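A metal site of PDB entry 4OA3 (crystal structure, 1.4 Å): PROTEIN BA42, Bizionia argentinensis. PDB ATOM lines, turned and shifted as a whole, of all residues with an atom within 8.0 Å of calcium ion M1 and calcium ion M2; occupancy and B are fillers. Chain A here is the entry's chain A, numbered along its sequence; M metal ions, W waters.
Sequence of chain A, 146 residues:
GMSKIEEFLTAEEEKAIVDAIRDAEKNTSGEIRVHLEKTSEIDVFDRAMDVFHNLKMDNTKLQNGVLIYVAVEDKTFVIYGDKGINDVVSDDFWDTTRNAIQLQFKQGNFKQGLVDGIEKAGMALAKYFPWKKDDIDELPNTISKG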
ATOM      1  N   ILE A  21     -26.276 -21.144   5.320  1.00  0.00           N
ATOM      2  CA  ILE A  21     -26.211 -20.240   4.172  1.00  0.00           C
ATOM      3  C   ILE A  21     -26.095 -18.802   4.670  1.00  0.00           C
ATOM      4  O   ILE A  21     -25.305 -18.012   4.146  1.00  0.00           O
ATOM      5  CB  ILE A  21     -27.426 -20.411   3.223  1.00  0.00           C
ATOM      6  CG1 ILE A  21     -27.342 -21.819   2.575  1.00  0.00           C
ATOM      7  CG2 ILE A  21     -27.424 -19.321   2.147  1.00  0.00           C
ATOM      8  CD1 ILE A  21     -28.544 -22.250   1.754  1.00  0.00           C
ATOM      9  N   ARG A  22     -26.940 -18.432   5.659  1.00  0.00           N
ATOM     10  CA  ARG A  22     -26.885 -17.058   6.172  1.00  0.00           C
ATOM     11  C   ARG A  22     -25.509 -16.715   6.719  1.00  0.00           C
ATOM     12  O   ARG A  22     -24.990 -15.633   6.430  1.00  0.00           O
ATOM     13  CB  ARG A  22     -27.935 -16.871   7.256  1.00  0.00           C
ATOM     14  CG  ARG A  22     -28.081 -15.450   7.736  1.00  0.00           C
ATOM     15  CD  ARG A  22     -29.354 -15.266   8.537  1.00  0.00           C
ATOM     16  NE  ARG A  22     -30.532 -15.628   7.757  1.00  0.00           N
ATOM     17  CZ  ARG A  22     -31.093 -14.882   6.796  1.00  0.00           C
ATOM     18  NH1 ARG A  22     -30.612 -13.681   6.506  1.00  0.00           N
ATOM     19  NH2 ARG A  22     -32.157 -15.328   6.150  1.00  0.00           N
ATOM     20  N   ALA A  24     -22.584 -18.231   5.870  1.00  0.00           N
ATOM     21  CA  ALA A  24     -21.643 -18.194   4.755  1.00  0.00           C
ATOM     22  C   ALA A  24     -21.709 -16.878   3.983  1.00  0.00           C
ATOM     23  O   ALA A  24     -20.691 -16.347   3.559  1.00  0.00           O
ATOM     24  CB  ALA A  24     -21.932 -19.358   3.812  1.00  0.00           C
ATOM     25  N   GLU A  25     -22.928 -16.340   3.797  1.00  0.00           N
ATOM     26  CA  GLU A  25     -23.107 -15.098   3.076  1.00  0.00           C
ATOM     27  C   GLU A  25     -22.704 -13.847   3.874  1.00  0.00           C
ATOM     28  O   GLU A  25     -22.789 -12.740   3.335  1.00  0.00           O
ATOM     29  CB  GLU A  25     -24.568 -14.986   2.587  1.00  0.00           C
ATOM     30  CG  GLU A  25     -24.888 -16.009   1.496  1.00  0.00           C
ATOM     31  CD  GLU A  25     -26.248 -15.853   0.858  1.00  0.00           C
ATOM     32  OE1 GLU A  25     -27.007 -14.948   1.294  1.00  0.00           O
ATOM     33  OE2 GLU A  25     -26.579 -16.631  -0.066  1.00  0.00           O
ATOM     34  N   LYS A  26     -22.204 -14.006   5.094  1.00  0.00           N
ATOM     35  CA  LYS A  26     -21.573 -12.896   5.820  1.00  0.00           C
ATOM     36  C   LYS A  26     -20.045 -12.918   5.562  1.00  0.00           C
ATOM     37  O   LYS A  26     -19.359 -12.001   5.996  1.00  0.00           O
ATOM     38  CB  LYS A  26     -21.832 -12.996   7.313  1.00  0.00           C
ATOM     39  CG  LYS A  26     -23.284 -12.818   7.714  1.00  0.00           C
ATOM     40  CD  LYS A  26     -23.430 -13.065   9.206  1.00  0.00           C
ATOM     41  CE  LYS A  26     -24.851 -13.063   9.654  1.00  0.00           C
ATOM     42  NZ  LYS A  26     -25.029 -13.811  10.921  1.00  0.00           N
ATOM     43  N   THR A  28     -18.782 -13.690   2.312  1.00  0.00           N
ATOM     44  CA  THR A  28     -18.586 -13.418   0.886  1.00  0.00           C
ATOM     45  C   THR A  28     -19.777 -12.681   0.304  1.00  0.00           C
ATOM     46  O   THR A  28     -20.861 -12.750   0.889  1.00  0.00           O
ATOM     47  CB  THR A  28     -18.434 -14.773   0.133  1.00  0.00           C
ATOM     48  OG1 THR A  28     -18.215 -14.541  -1.259  1.00  0.00           O
ATOM     49  CG2 THR A  28     -19.675 -15.691   0.300  1.00  0.00           C
ATOM     50  N   SER A  29     -19.584 -12.002  -0.828  1.00  0.00           N
ATOM     51  CA  SER A  29     -20.679 -11.419  -1.588  1.00  0.00           C
ATOM     52  C   SER A  29     -21.324 -12.513  -2.465  1.00  0.00           C
ATOM     53  O   SER A  29     -22.376 -12.265  -3.064  1.00  0.00           O
ATOM     54  CB  SER A  29     -20.210 -10.275  -2.479  1.00  0.00           C
ATOM     55  OG  SER A  29     -19.407 -10.751  -3.531  1.00  0.00           O
ATOM     56  N   GLY A  30     -20.741 -13.713  -2.528  1.00  0.00           N
ATOM     57  CA  GLY A  30     -21.348 -14.822  -3.233  1.00  0.00           C
ATOM     58  C   GLY A  30     -22.653 -15.253  -2.574  1.00  0.00           C
ATOM     59  O   GLY A  30     -22.908 -14.991  -1.400  1.00  0.00           O
ATOM     60  N   GLU A  31     -23.521 -15.841  -3.391  1.00  0.00           N
ATOM     61  CA  GLU A  31     -24.837 -16.274  -2.945  1.00  0.00           C
ATOM     62  C   GLU A  31     -24.984 -17.753  -3.133  1.00  0.00           C
ATOM     63  O   GLU A  31     -24.598 -18.264  -4.189  1.00  0.00           O
ATOM     64  CB  GLU A  31     -25.891 -15.538  -3.720  1.00  0.00           C
ATOM     65  CG  GLU A  31     -25.930 -14.042  -3.443  1.00  0.00           C
ATOM     66  CD  GLU A  31     -26.796 -13.615  -2.274  1.00  0.00           C
ATOM     67  OE1 GLU A  31     -27.779 -14.336  -1.979  1.00  0.00           O
ATOM     68  OE2 GLU A  31     -26.490 -12.566  -1.636  1.00  0.00           O
ATOM     69  N   ILE A  32     -25.488 -18.458  -2.129  1.00  0.00           N
ATOM     70  CA  ILE A  32     -25.554 -19.913  -2.152  1.00  0.00           C
ATOM     71  C   ILE A  32     -26.961 -20.419  -2.006  1.00  0.00           C
ATOM     72  O   ILE A  32     -27.693 -19.957  -1.152  1.00  0.00           O
ATOM     73  CB  ILE A  32     -24.682 -20.510  -1.001  1.00  0.00           C
ATOM     74  CG1 ILE A  32     -23.219 -20.098  -1.155  1.00  0.00           C
ATOM     75  CG2 ILE A  32     -24.835 -22.042  -0.936  1.00  0.00           C
ATOM     76  CD1 ILE A  32     -22.435 -20.195   0.100  1.00  0.00           C
ATOM     77  N   ARG A  33     -27.362 -21.413  -2.849  1.00  0.00           N
ATOM     78  CA  ARG A  33     -28.606 -22.151  -2.646  1.00  0.00           C
ATOM     79  C   ARG A  33     -28.385 -23.624  -2.805  1.00  0.00           C
ATOM     80  O   ARG A  33     -27.437 -24.067  -3.474  1.00  0.00           O
ATOM     81  CB  ARG A  33     -29.728 -21.748  -3.614  1.00  0.00           C
ATOM     82  CG  ARG A  33     -30.129 -20.289  -3.454  1.00  0.00           C
ATOM     83  CD  ARG A  33     -31.423 -19.939  -4.148  1.00  0.00           C
ATOM     84  NE  ARG A  33     -32.541 -20.627  -3.492  1.00  0.00           N
ATOM     85  CZ  ARG A  33     -33.758 -20.699  -3.984  1.00  0.00           C
ATOM     86  NH1 ARG A  33     -34.048 -20.136  -5.147  1.00  0.00           N
ATOM     87  NH2 ARG A  33     -34.704 -21.358  -3.329  1.00  0.00           N
ATOM     88  N   THR A  60     -27.491 -11.907  -9.724  1.00  0.00           N
ATOM     89  CA  THR A  60     -26.542 -11.363  -8.762  1.00  0.00           C
ATOM     90  C   THR A  60     -25.717 -10.334  -9.542  1.00  0.00           C
ATOM     91  O   THR A  60     -25.428 -10.542 -10.724  1.00  0.00           O
ATOM     92  CB  THR A  60     -25.663 -12.449  -8.124  1.00  0.00           C
ATOM     93  OG1 THR A  60     -24.757 -13.004  -9.087  1.00  0.00           O
ATOM     94  CG2 THR A  60     -26.471 -13.517  -7.412  1.00  0.00           C
ATOM     95  N   ASN A  64     -22.093 -14.315  -9.212  1.00  0.00           N
ATOM     96  CA  ASN A  64     -21.430 -15.162  -8.260  1.00  0.00           C
ATOM     97  C   ASN A  64     -22.355 -16.014  -7.380  1.00  0.00           C
ATOM     98  O   ASN A  64     -22.047 -16.291  -6.238  1.00  0.00           O
ATOM     99  CB  ASN A  64     -20.422 -14.369  -7.440  1.00  0.00           C
ATOM    100  CG  ASN A  64     -21.045 -13.277  -6.623  1.00  0.00           C
ATOM    101  OD1 ASN A  64     -22.207 -12.973  -6.742  1.00  0.00           O
ATOM    102  ND2 ASN A  64     -20.263 -12.699  -5.721  1.00  0.00           N
ATOM    103  N   TRP A 131     -16.976 -10.041   1.232  1.00  0.00           N
ATOM    104  CA  TRP A 131     -18.200  -9.435   1.731  1.00  0.00           C
ATOM    105  C   TRP A 131     -17.967  -7.919   1.893  1.00  0.00           C
ATOM    106  O   TRP A 131     -16.874  -7.499   2.282  1.00  0.00           O
ATOM    107  CB  TRP A 131     -18.574 -10.051   3.076  1.00  0.00           C
ATOM    108  CG  TRP A 131     -19.825  -9.514   3.681  1.00  0.00           C
ATOM    109  CD1 TRP A 131     -21.092  -9.968   3.504  1.00  0.00           C
ATOM    110  CD2 TRP A 131     -19.909  -8.432   4.629  1.00  0.00           C
ATOM    111  NE1 TRP A 131     -21.979  -9.203   4.235  1.00  0.00           N
ATOM    112  CE2 TRP A 131     -21.274  -8.244   4.922  1.00  0.00           C
ATOM    113  CE3 TRP A 131     -18.962  -7.598   5.239  1.00  0.00           C
ATOM    114  CZ2 TRP A 131     -21.713  -7.282   5.829  1.00  0.00           C
ATOM    115  CZ3 TRP A 131     -19.409  -6.608   6.102  1.00  0.00           C
ATOM    116  CH2 TRP A 131     -20.761  -6.498   6.436  1.00  0.00           C
ATOM    117  N   LYS A 132     -18.978  -7.131   1.534  1.00  0.00           N
ATOM    118  CA  LYS A 132     -18.950  -5.671   1.614  1.00  0.00           C
ATOM    119  C   LYS A 132     -20.049  -5.219   2.553  1.00  0.00           C
ATOM    120  O   LYS A 132     -21.099  -5.863   2.638  1.00  0.00           O
ATOM    121  CB  LYS A 132     -19.187  -5.039   0.243  1.00  0.00           C
ATOM    122  CG  LYS A 132     -18.238  -5.509  -0.854  1.00  0.00           C
ATOM    123  CD  LYS A 132     -16.796  -5.158  -0.583  1.00  0.00           C
ATOM    124  CE  LYS A 132     -15.911  -5.439  -1.772  1.00  0.00           C
ATOM    125  NZ  LYS A 132     -16.240  -4.590  -2.953  1.00  0.00           N
ATOM    126  N   ASP A 134     -22.451  -2.992   2.525  1.00  0.00           N
ATOM    127  CA  ASP A 134     -23.776  -2.773   1.949  1.00  0.00           C
ATOM    128  C   ASP A 134     -24.237  -4.025   1.154  1.00  0.00           C
ATOM    129  O   ASP A 134     -25.018  -3.915   0.202  1.00  0.00           O
ATOM    130  CB  ASP A 134     -23.774  -1.498   1.069  1.00  0.00           C
ATOM    131  CG  ASP A 134     -22.633  -1.400   0.068  1.00  0.00           C
ATOM    132  OD1 ASP A 134     -21.677  -2.198   0.188  1.00  0.00           O
ATOM    133  OD2 ASP A 134     -22.670  -0.499  -0.796  1.00  0.00           O
ATOM    134  N   ASP A 135     -23.774  -5.222   1.575  1.00  0.00           N
ATOM    135  CA  ASP A 135     -24.168  -6.465   0.924  1.00  0.00           C
ATOM    136  C   ASP A 135     -25.672  -6.555   0.839  1.00  0.00           C
ATOM    137  O   ASP A 135     -26.366  -6.230   1.803  1.00  0.00           O
ATOM    138  CB  ASP A 135     -23.683  -7.684   1.737  1.00  0.00           C
ATOM    139  CG  ASP A 135     -24.115  -9.004   1.094  1.00  0.00           C
ATOM    140  OD1 ASP A 135     -23.423  -9.451   0.166  1.00  0.00           O
ATOM    141  OD2 ASP A 135     -25.127  -9.572   1.543  1.00  0.00           O
ATOM    142  N   ILE A 136     -26.156  -7.044  -0.285  1.00  0.00           N
ATOM    143  CA  ILE A 136     -27.573  -7.300  -0.531  1.00  0.00           C
ATOM    144  C   ILE A 136     -27.747  -8.838  -0.471  1.00  0.00           C
ATOM    145  O   ILE A 136     -26.895  -9.553  -0.998  1.00  0.00           O
ATOM    146  CB  ILE A 136     -27.946  -6.770  -1.929  1.00  0.00           C
ATOM    147  CG1 ILE A 136     -27.784  -5.212  -1.982  1.00  0.00           C
ATOM    148  CG2 ILE A 136     -29.383  -7.208  -2.330  1.00  0.00           C
ATOM    149  CD1 ILE A 136     -28.016  -4.644  -3.311  1.00  0.00           C
ATOM    150  N   ASP A 137     -28.841  -9.331   0.124  1.00  0.00           N
ATOM    151  CA  ASP A 137     -29.136 -10.775   0.116  1.00  0.00           C
ATOM    152  C   ASP A 137     -29.903 -10.966  -1.215  1.00  0.00           C
ATOM    153  O   ASP A 137     -31.102 -10.738  -1.302  1.00  0.00           O
ATOM    154  CB  ASP A 137     -29.947 -11.183   1.337  1.00  0.00           C
ATOM    155  CG  ASP A 137     -30.021 -12.673   1.555  1.00  0.00           C
ATOM    156  OD1 ASP A 137     -29.730 -13.442   0.595  1.00  0.00           O
ATOM    157  OD2 ASP A 137     -30.380 -13.088   2.671  1.00  0.00           O
ATOM    158  N   GLU A 138     -29.140 -11.211  -2.276  1.00  0.00           N
ATOM    159  CA  GLU A 138     -29.648 -11.226  -3.650  1.00  0.00           C
ATOM    160  C   GLU A 138     -30.521 -12.396  -4.026  1.00  0.00           C
ATOM    161  O   GLU A 138     -31.450 -12.225  -4.814  1.00  0.00           O
ATOM    162  CB  GLU A 138     -28.471 -11.106  -4.626  1.00  0.00           C
ATOM    163  CG  GLU A 138     -27.708  -9.784  -4.510  1.00  0.00           C
ATOM    164  CD  GLU A 138     -26.459  -9.720  -5.349  1.00  0.00           C
ATOM    165  OE1 GLU A 138     -25.513 -10.481  -5.058  1.00  0.00           O
ATOM    166  OE2 GLU A 138     -26.396  -8.861  -6.273  1.00  0.00           O
ATOM    167  N   LEU A 139     -30.232 -13.568  -3.466  1.00  0.00           N
ATOM    168  CA  LEU A 139     -30.987 -14.774  -3.749  1.00  0.00           C
ATOM    169  C   LEU A 139     -31.559 -15.307  -2.458  1.00  0.00           C
ATOM    170  O   LEU A 139     -30.893 -15.269  -1.431  1.00  0.00           O
ATOM    171  CB  LEU A 139     -30.106 -15.863  -4.357  1.00  0.00           C
ATOM    172  CG  LEU A 139     -29.339 -15.476  -5.632  1.00  0.00           C
ATOM    173  CD1 LEU A 139     -28.470 -16.645  -6.121  1.00  0.00           C
ATOM    174  CD2 LEU A 139     -30.262 -15.016  -6.743  1.00  0.00           C
ATOM    175  N   PRO A 140     -32.788 -15.870  -2.466  1.00  0.00           N
ATOM    176  CA  PRO A 140     -33.314 -16.478  -1.247  1.00  0.00           C
ATOM    177  C   PRO A 140     -32.463 -17.636  -0.737  1.00  0.00           C
ATOM    178  O   PRO A 140     -31.749 -18.290  -1.516  1.00  0.00           O
ATOM    179  CB  PRO A 140     -34.724 -16.933  -1.640  1.00  0.00           C
ATOM    180  CG  PRO A 140     -34.751 -16.950  -3.037  1.00  0.00           C
ATOM    181  CD  PRO A 140     -33.691 -16.046  -3.600  1.00  0.00           C
ATOM    182  N   ASN A 141     -32.484 -17.838   0.578  1.00  0.00           N
ATOM    183  CA  ASN A 141     -31.683 -18.890   1.202  1.00  0.00           C
ATOM    184  C   ASN A 141     -32.487 -20.179   1.347  1.00  0.00           C
ATOM    185  O   ASN A 141     -31.927 -21.177   1.745  1.00  0.00           O
ATOM    186  CB  ASN A 141     -31.158 -18.434   2.535  1.00  0.00           C
ATOM    187  CG  ASN A 141     -30.260 -17.221   2.474  1.00  0.00           C
ATOM    188  OD1 ASN A 141     -29.776 -16.798   1.426  1.00  0.00           O
ATOM    189  ND2 ASN A 141     -29.944 -16.717   3.672  1.00  0.00           N
ATOM    190  N   THR A 142     -33.762 -20.143   0.940  1.00  0.00           N
ATOM    191  CA  THR A 142     -34.692 -21.287   0.947  1.00  0.00           C
ATOM    192  C   THR A 142     -34.089 -22.458   0.219  1.00  0.00           C
ATOM    193  O   THR A 142     -33.557 -22.276  -0.885  1.00  0.00           O
ATOM    194  CB  THR A 142     -35.947 -20.902   0.111  1.00  0.00           C
ATOM    195  OG1 THR A 142     -36.333 -19.581   0.361  1.00  0.00           O
ATOM    196  CG2 THR A 142     -37.141 -21.804   0.324  1.00  0.00           C
HETATM  197 CA    CA M   1     -25.202 -11.100  -0.354  1.00  0.00          CA
HETATM  198 CA    CA M   2     -28.846 -15.516  -0.223  1.00  0.00          CA
HETATM  199  O   HOH W   1     -29.027 -17.563  -1.447  1.00  0.00           O
HETATM  200  O   HOH W   2     -23.542 -12.764   0.040  1.00  0.00           O
HETATM  201  O   HOH W   3     -26.505 -12.178   1.458  1.00  0.00           O
HETATM  202  O   HOH W   4     -24.282 -10.567  -2.561  1.00  0.00           O
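Within 4 Å of calcium ion M1: Glu 31, Asp 135, Ile 136 and Asp 137.
Water W4 bridges O of Ser 29 (2.6 Å) and OE1 of Glu 138 (2.8 Å). Water W1 lies within hydrogen-bond range of O of Ile 32 and O of Pro 140.
Calcium ion M2 is bound by the side-chain amide oxygen (OD1) of Asn 141 (2.3 Å), the side-chain carboxylate (OE1) of Glu 31 (2.4 Å), the backbone carbonyl oxygen (O) of Leu 139 (2.4 Å), water W1 (2.4 Å), the side-chain carboxylate (OD1) of Asp 137 (2.4 Å), the side-chain carboxylate (OE1) of Glu 25 (2.5 Å) and the side-chain carboxylate (OE2) of Glu 25 (2.5 Å).
The nearest printed residue that does not touch calcium ion M2 is Pro 140 (4.2 Å).
The side-chain carboxylate (OE2) of Glu 31 lies close to the backbone NH (N) of Glu 138 (3.0 Å). The backbone NH (N) of Glu 31 sits at hydrogen-bond distance from the backbone carbonyl oxygen (O) of Asn 64 (3.2 Å). OE2 of Glu 25 sits close to N of Ile 32, 3.0 Å away. The guanidinium group (NH1) of Arg 22 is in salt-bridge range of the side-chain carboxylate (OD2) of Asp 137, at 3.9 Å.
Calcium ion M1 is bound by the side-chain carboxylate (OE2) of Glu 31 (2.3 Å), the backbone carbonyl oxygen (O) of Ile 136 (2.4 Å), water W2 (2.4 Å), the side-chain carboxylate (OD2) of Asp 135 (2.4 Å), water W4 (2.4 Å), water W3 (2.5 Å) and the side-chain carboxylate (OD1) of Asp 135 (2.5 Å).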
